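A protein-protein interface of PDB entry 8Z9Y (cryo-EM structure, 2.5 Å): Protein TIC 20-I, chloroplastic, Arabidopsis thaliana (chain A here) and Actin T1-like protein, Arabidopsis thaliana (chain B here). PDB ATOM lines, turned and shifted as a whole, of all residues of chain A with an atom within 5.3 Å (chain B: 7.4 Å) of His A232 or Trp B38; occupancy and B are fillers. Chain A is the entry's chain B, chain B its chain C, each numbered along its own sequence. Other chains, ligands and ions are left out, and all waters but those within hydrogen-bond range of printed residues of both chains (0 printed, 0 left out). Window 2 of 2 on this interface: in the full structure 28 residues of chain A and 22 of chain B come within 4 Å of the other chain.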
ATOM      1  N   LEU A 149      -1.166  16.117  -1.314  1.00  0.00           N
ATOM      2  CA  LEU A 149      -2.351  15.268  -1.283  1.00  0.00           C
ATOM      3  C   LEU A 149      -2.175  13.938  -1.997  1.00  0.00           C
ATOM      4  O   LEU A 149      -2.651  12.914  -1.502  1.00  0.00           O
ATOM      5  CB  LEU A 149      -3.538  16.018  -1.897  1.00  0.00           C
ATOM      6  CG  LEU A 149      -4.938  15.460  -1.656  1.00  0.00           C
ATOM      7  CD1 LEU A 149      -5.905  16.588  -1.341  1.00  0.00           C
ATOM      8  CD2 LEU A 149      -5.416  14.671  -2.865  1.00  0.00           C
ATOM      9  N   GLY A 227      -3.925  26.719   0.916  1.00  0.00           N
ATOM     10  CA  GLY A 227      -4.793  26.233   1.965  1.00  0.00           C
ATOM     11  C   GLY A 227      -5.441  24.908   1.609  1.00  0.00           C
ATOM     12  O   GLY A 227      -5.247  24.339   0.533  1.00  0.00           O
ATOM     13  N   LYS A 228      -6.240  24.407   2.552  1.00  0.00           N
ATOM     14  CA  LYS A 228      -6.872  23.102   2.400  1.00  0.00           C
ATOM     15  C   LYS A 228      -7.916  23.070   1.292  1.00  0.00           C
ATOM     16  O   LYS A 228      -8.353  21.979   0.911  1.00  0.00           O
ATOM     17  CB  LYS A 228      -7.507  22.676   3.724  1.00  0.00           C
ATOM     18  CG  LYS A 228      -7.463  21.180   3.980  1.00  0.00           C
ATOM     19  CD  LYS A 228      -7.946  20.845   5.380  1.00  0.00           C
ATOM     20  CE  LYS A 228      -8.400  19.398   5.474  1.00  0.00           C
ATOM     21  NZ  LYS A 228      -7.497  18.485   4.719  1.00  0.00           N
ATOM     22  N   PHE A 229      -8.328  24.226   0.773  1.00  0.00           N
ATOM     23  CA  PHE A 229      -9.289  24.278  -0.321  1.00  0.00           C
ATOM     24  C   PHE A 229      -8.614  24.279  -1.687  1.00  0.00           C
ATOM     25  O   PHE A 229      -9.073  23.588  -2.607  1.00  0.00           O
ATOM     26  CB  PHE A 229     -10.174  25.519  -0.180  1.00  0.00           C
ATOM     27  CG  PHE A 229     -11.065  25.767  -1.362  1.00  0.00           C
ATOM     28  CD1 PHE A 229     -12.062  24.867  -1.697  1.00  0.00           C
ATOM     29  CD2 PHE A 229     -10.905  26.901  -2.139  1.00  0.00           C
ATOM     30  CE1 PHE A 229     -12.883  25.095  -2.785  1.00  0.00           C
ATOM     31  CE2 PHE A 229     -11.721  27.135  -3.227  1.00  0.00           C
ATOM     32  CZ  PHE A 229     -12.712  26.231  -3.551  1.00  0.00           C
ATOM     33  N   GLY A 230      -7.530  25.042  -1.834  1.00  0.00           N
ATOM     34  CA  GLY A 230      -6.870  25.136  -3.126  1.00  0.00           C
ATOM     35  C   GLY A 230      -6.304  23.809  -3.591  1.00  0.00           C
ATOM     36  O   GLY A 230      -6.440  23.437  -4.759  1.00  0.00           O
ATOM     37  N   MET A 231      -5.661  23.075  -2.681  1.00  0.00           N
ATOM     38  CA  MET A 231      -5.083  21.788  -3.055  1.00  0.00           C
ATOM     39  C   MET A 231      -6.167  20.777  -3.415  1.00  0.00           C
ATOM     40  O   MET A 231      -6.004  19.995  -4.360  1.00  0.00           O
ATOM     41  CB  MET A 231      -4.177  21.270  -1.933  1.00  0.00           C
ATOM     42  CG  MET A 231      -4.860  20.474  -0.829  1.00  0.00           C
ATOM     43  SD  MET A 231      -3.781  20.217   0.593  1.00  0.00           S
ATOM     44  CE  MET A 231      -4.684  18.958   1.489  1.00  0.00           C
ATOM     45  N   HIS A 232      -7.289  20.793  -2.690  1.00  0.00           N
ATOM     46  CA  HIS A 232      -8.372  19.859  -2.979  1.00  0.00           C
ATOM     47  C   HIS A 232      -9.038  20.187  -4.309  1.00  0.00           C
ATOM     48  O   HIS A 232      -9.476  19.283  -5.029  1.00  0.00           O
ATOM     49  CB  HIS A 232      -9.394  19.876  -1.845  1.00  0.00           C
ATOM     50  CG  HIS A 232      -9.006  19.031  -0.673  1.00  0.00           C
ATOM     51  ND1 HIS A 232      -8.346  19.540   0.423  1.00  0.00           N
ATOM     52  CD2 HIS A 232      -9.180  17.711  -0.430  1.00  0.00           C
ATOM     53  CE1 HIS A 232      -8.132  18.571   1.295  1.00  0.00           C
ATOM     54  NE2 HIS A 232      -8.626  17.451   0.801  1.00  0.00           N
ATOM     55  N   PHE A 233      -9.137  21.473  -4.643  1.00  0.00           N
ATOM     56  CA  PHE A 233      -9.627  21.858  -5.962  1.00  0.00           C
ATOM     57  C   PHE A 233      -8.659  21.416  -7.054  1.00  0.00           C
ATOM     58  O   PHE A 233      -9.065  20.853  -8.082  1.00  0.00           O
ATOM     59  CB  PHE A 233      -9.848  23.372  -5.998  1.00  0.00           C
ATOM     60  CG  PHE A 233      -9.773  23.976  -7.374  1.00  0.00           C
ATOM     61  CD1 PHE A 233     -10.889  24.012  -8.190  1.00  0.00           C
ATOM     62  CD2 PHE A 233      -8.591  24.533  -7.837  1.00  0.00           C
ATOM     63  CE1 PHE A 233     -10.822  24.575  -9.450  1.00  0.00           C
ATOM     64  CE2 PHE A 233      -8.520  25.095  -9.096  1.00  0.00           C
ATOM     65  CZ  PHE A 233      -9.636  25.116  -9.903  1.00  0.00           C
ATOM     66  N   TRP A 234      -7.362  21.641  -6.835  1.00  0.00           N
ATOM     67  CA  TRP A 234      -6.393  21.451  -7.903  1.00  0.00           C
ATOM     68  C   TRP A 234      -6.101  19.983  -8.179  1.00  0.00           C
ATOM     69  O   TRP A 234      -5.843  19.627  -9.331  1.00  0.00           O
ATOM     70  CB  TRP A 234      -5.099  22.197  -7.581  1.00  0.00           C
ATOM     71  CG  TRP A 234      -5.027  23.515  -8.279  1.00  0.00           C
ATOM     72  CD1 TRP A 234      -5.121  24.750  -7.711  1.00  0.00           C
ATOM     73  CD2 TRP A 234      -4.893  23.730  -9.688  1.00  0.00           C
ATOM     74  NE1 TRP A 234      -5.028  25.723  -8.676  1.00  0.00           N
ATOM     75  CE2 TRP A 234      -4.890  25.122  -9.899  1.00  0.00           C
ATOM     76  CE3 TRP A 234      -4.762  22.881 -10.791  1.00  0.00           C
ATOM     77  CZ2 TRP A 234      -4.765  25.684 -11.167  1.00  0.00           C
ATOM     78  CZ3 TRP A 234      -4.637  23.441 -12.047  1.00  0.00           C
ATOM     79  CH2 TRP A 234      -4.640  24.827 -12.226  1.00  0.00           C
ATOM     80  N   THR A 235      -6.133  19.117  -7.161  1.00  0.00           N
ATOM     81  CA  THR A 235      -5.941  17.695  -7.435  1.00  0.00           C
ATOM     82  C   THR A 235      -7.056  17.157  -8.326  1.00  0.00           C
ATOM     83  O   THR A 235      -6.796  16.427  -9.293  1.00  0.00           O
ATOM     84  CB  THR A 235      -5.849  16.896  -6.130  1.00  0.00           C
ATOM     85  OG1 THR A 235      -5.797  15.495  -6.429  1.00  0.00           O
ATOM     86  CG2 THR A 235      -7.038  17.168  -5.220  1.00  0.00           C
ATOM     87  N   ALA A 236      -8.303  17.533  -8.030  1.00  0.00           N
ATOM     88  CA  ALA A 236      -9.423  17.116  -8.864  1.00  0.00           C
ATOM     89  C   ALA A 236      -9.299  17.681 -10.271  1.00  0.00           C
ATOM     90  O   ALA A 236      -9.528  16.968 -11.256  1.00  0.00           O
ATOM     91  CB  ALA A 236     -10.743  17.548  -8.228  1.00  0.00           C
ATOM     92  N   SER B  30     -13.514  12.597 -10.484  1.00  0.00           N
ATOM     93  CA  SER B  30     -12.436  13.411  -9.928  1.00  0.00           C
ATOM     94  C   SER B  30     -12.932  14.265  -8.767  1.00  0.00           C
ATOM     95  O   SER B  30     -12.280  14.343  -7.716  1.00  0.00           O
ATOM     96  CB  SER B  30     -11.826  14.288 -11.020  1.00  0.00           C
ATOM     97  OG  SER B  30     -10.975  13.531 -11.862  1.00  0.00           O
ATOM     98  N   ALA B  31     -14.093  14.905  -8.933  1.00  0.00           N
ATOM     99  CA  ALA B  31     -14.644  15.715  -7.849  1.00  0.00           C
ATOM    100  C   ALA B  31     -14.967  14.862  -6.628  1.00  0.00           C
ATOM    101  O   ALA B  31     -14.677  15.253  -5.488  1.00  0.00           O
ATOM    102  CB  ALA B  31     -15.888  16.460  -8.330  1.00  0.00           C
ATOM    103  N   ALA B  32     -15.563  13.687  -6.847  1.00  0.00           N
ATOM    104  CA  ALA B  32     -15.898  12.804  -5.737  1.00  0.00           C
ATOM    105  C   ALA B  32     -14.645  12.310  -5.029  1.00  0.00           C
ATOM    106  O   ALA B  32     -14.627  12.192  -3.800  1.00  0.00           O
ATOM    107  CB  ALA B  32     -16.734  11.627  -6.237  1.00  0.00           C
ATOM    108  N   PHE B  33     -13.590  12.005  -5.788  1.00  0.00           N
ATOM    109  CA  PHE B  33     -12.332  11.591  -5.180  1.00  0.00           C
ATOM    110  C   PHE B  33     -11.741  12.707  -4.333  1.00  0.00           C
ATOM    111  O   PHE B  33     -11.230  12.458  -3.234  1.00  0.00           O
ATOM    112  CB  PHE B  33     -11.343  11.157  -6.259  1.00  0.00           C
ATOM    113  CG  PHE B  33      -9.936  11.005  -5.763  1.00  0.00           C
ATOM    114  CD1 PHE B  33      -9.586   9.937  -4.954  1.00  0.00           C
ATOM    115  CD2 PHE B  33      -8.963  11.928  -6.103  1.00  0.00           C
ATOM    116  CE1 PHE B  33      -8.292   9.794  -4.493  1.00  0.00           C
ATOM    117  CE2 PHE B  33      -7.668  11.791  -5.644  1.00  0.00           C
ATOM    118  CZ  PHE B  33      -7.332  10.722  -4.838  1.00  0.00           C
ATOM    119  N   SER B  34     -11.793  13.946  -4.828  1.00  0.00           N
ATOM    120  CA  SER B  34     -11.299  15.069  -4.036  1.00  0.00           C
ATOM    121  C   SER B  34     -12.081  15.213  -2.736  1.00  0.00           C
ATOM    122  O   SER B  34     -11.491  15.397  -1.662  1.00  0.00           O
ATOM    123  CB  SER B  34     -11.370  16.359  -4.851  1.00  0.00           C
ATOM    124  OG  SER B  34     -11.438  17.491  -4.003  1.00  0.00           O
ATOM    125  N   VAL B  35     -13.411  15.115  -2.808  1.00  0.00           N
ATOM    126  CA  VAL B  35     -14.228  15.239  -1.602  1.00  0.00           C
ATOM    127  C   VAL B  35     -13.928  14.106  -0.625  1.00  0.00           C
ATOM    128  O   VAL B  35     -13.804  14.325   0.587  1.00  0.00           O
ATOM    129  CB  VAL B  35     -15.723  15.292  -1.968  1.00  0.00           C
ATOM    130  CG1 VAL B  35     -16.572  15.362  -0.712  1.00  0.00           C
ATOM    131  CG2 VAL B  35     -16.003  16.489  -2.859  1.00  0.00           C
ATOM    132  N   LEU B  36     -13.810  12.876  -1.134  1.00  0.00           N
ATOM    133  CA  LEU B  36     -13.530  11.736  -0.268  1.00  0.00           C
ATOM    134  C   LEU B  36     -12.167  11.868   0.399  1.00  0.00           C
ATOM    135  O   LEU B  36     -12.013  11.542   1.581  1.00  0.00           O
ATOM    136  CB  LEU B  36     -13.613  10.437  -1.069  1.00  0.00           C
ATOM    137  CG  LEU B  36     -15.020   9.982  -1.459  1.00  0.00           C
ATOM    138  CD1 LEU B  36     -14.958   8.758  -2.357  1.00  0.00           C
ATOM    139  CD2 LEU B  36     -15.857   9.704  -0.221  1.00  0.00           C
ATOM    140  N   THR B  37     -11.164  12.337  -0.347  1.00  0.00           N
ATOM    141  CA  THR B  37      -9.854  12.573   0.247  1.00  0.00           C
ATOM    142  C   THR B  37      -9.932  13.649   1.323  1.00  0.00           C
ATOM    143  O   THR B  37      -9.275  13.546   2.365  1.00  0.00           O
ATOM    144  CB  THR B  37      -8.848  12.962  -0.836  1.00  0.00           C
ATOM    145  OG1 THR B  37      -8.545  11.815  -1.638  1.00  0.00           O
ATOM    146  CG2 THR B  37      -7.565  13.472  -0.210  1.00  0.00           C
ATOM    147  N   TRP B  38     -10.740  14.688   1.089  1.00  0.00           N
ATOM    148  CA  TRP B  38     -10.996  15.667   2.141  1.00  0.00           C
ATOM    149  C   TRP B  38     -11.572  14.992   3.380  1.00  0.00           C
ATOM    150  O   TRP B  38     -11.190  15.319   4.510  1.00  0.00           O
ATOM    151  CB  TRP B  38     -11.944  16.753   1.629  1.00  0.00           C
ATOM    152  CG  TRP B  38     -11.984  17.999   2.474  1.00  0.00           C
ATOM    153  CD1 TRP B  38     -12.060  18.070   3.836  1.00  0.00           C
ATOM    154  CD2 TRP B  38     -11.961  19.353   2.006  1.00  0.00           C
ATOM    155  NE1 TRP B  38     -12.078  19.381   4.243  1.00  0.00           N
ATOM    156  CE2 TRP B  38     -12.019  20.188   3.138  1.00  0.00           C
ATOM    157  CE3 TRP B  38     -11.896  19.939   0.738  1.00  0.00           C
ATOM    158  CZ2 TRP B  38     -12.013  21.576   3.042  1.00  0.00           C
ATOM    159  CZ3 TRP B  38     -11.888  21.319   0.646  1.00  0.00           C
ATOM    160  CH2 TRP B  38     -11.947  22.121   1.790  1.00  0.00           C
ATOM    161  N   VAL B  39     -12.486  14.041   3.186  1.00  0.00           N
ATOM    162  CA  VAL B  39     -13.080  13.340   4.322  1.00  0.00           C
ATOM    163  C   VAL B  39     -12.030  12.499   5.042  1.00  0.00           C
ATOM    164  O   VAL B  39     -11.916  12.540   6.273  1.00  0.00           O
ATOM    165  CB  VAL B  39     -14.274  12.486   3.858  1.00  0.00           C
ATOM    166  CG1 VAL B  39     -14.475  11.291   4.780  1.00  0.00           C
ATOM    167  CG2 VAL B  39     -15.535  13.333   3.794  1.00  0.00           C
ATOM    168  N   ASN B  40     -11.243  11.729   4.289  1.00  0.00           N
ATOM    169  CA  ASN B  40     -10.246  10.820   4.857  1.00  0.00           C
ATOM    170  C   ASN B  40      -8.902  11.056   4.179  1.00  0.00           C
ATOM    171  O   ASN B  40      -8.623  10.491   3.114  1.00  0.00           O
ATOM    172  CB  ASN B  40     -10.682   9.365   4.712  1.00  0.00           C
ATOM    173  CG  ASN B  40      -9.725   8.402   5.384  1.00  0.00           C
ATOM    174  OD1 ASN B  40      -8.932   8.792   6.240  1.00  0.00           O
ATOM    175  ND2 ASN B  40      -9.795   7.134   4.998  1.00  0.00           N
ATOM    176  N   PRO B  41      -8.042  11.891   4.770  1.00  0.00           N
ATOM    177  CA  PRO B  41      -6.743  12.164   4.135  1.00  0.00           C
ATOM    178  C   PRO B  41      -5.801  10.973   4.133  1.00  0.00           C
ATOM    179  O   PRO B  41      -4.987  10.848   3.209  1.00  0.00           O
ATOM    180  CB  PRO B  41      -6.176  13.324   4.968  1.00  0.00           C
ATOM    181  CG  PRO B  41      -7.312  13.806   5.829  1.00  0.00           C
ATOM    182  CD  PRO B  41      -8.213  12.636   6.025  1.00  0.00           C
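A ring nitrogen (NE2) of His A232 sits close to the backbone NH of Trp B38 (3.5 Å). The side-chain hydroxyl (OG) of Ser B34 sits at hydrogen-bond distance from the backbone carbonyl oxygen (O) of His A232, at 2.8 Å.
O of Phe B33 sits at hydrogen-bond distance from OG1 of Thr B37, at 3.2 Å. ND1 of His A232 is in hydrogen-bond range of O of Lys A228 (2.5 Å).
Thr B37 touches Leu A149. Lys A228 touches Trp B38. CB of Ser B30 touches O of Ala A236 (3.5 Å). Ala A236 touches Ser B34 (CB to CB, 3.6 Å).
Of the printed residues of chain B, Leu A149 touches Thr B37 (3.6 Å). Of the printed residues of chain B, Lys A228 touches Trp B38. His A232 touches just these residues of chain B: Ser B34 and Trp B38. Printed residues of chain A within 4 Å of Ser B30: Ala A236. Of the printed residues of chain A, Thr B37 touches Leu A149. Trp B38 touches two residues of chain A. Val B39 touches none of the printed residues of chain A. Pro B41 touches none of the printed residues of chain A. The nearest residue of chain B that does not touch His A232 is Thr B37 (4.1 Å). The nearest residue of chain A that does not touch Trp B38 is Phe A229 (4.02 Å).
Of the 12 printed residues of chain B, 4 touch a printed residue of chain A. Of the 11 printed residues of chain A, 4 touch a printed residue of chain B. Hydrophobic or aromatic side chains of chain A within 4 Å of the printed part of chain B: Leu A149, His A232 and Ala A236. Among the printed residues, 6 pairs touch across the chains. Among the printed residues, no Asp or Glu carboxylate lies within 4 Å of a Lys or Arg side-chain nitrogen of the other chain.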
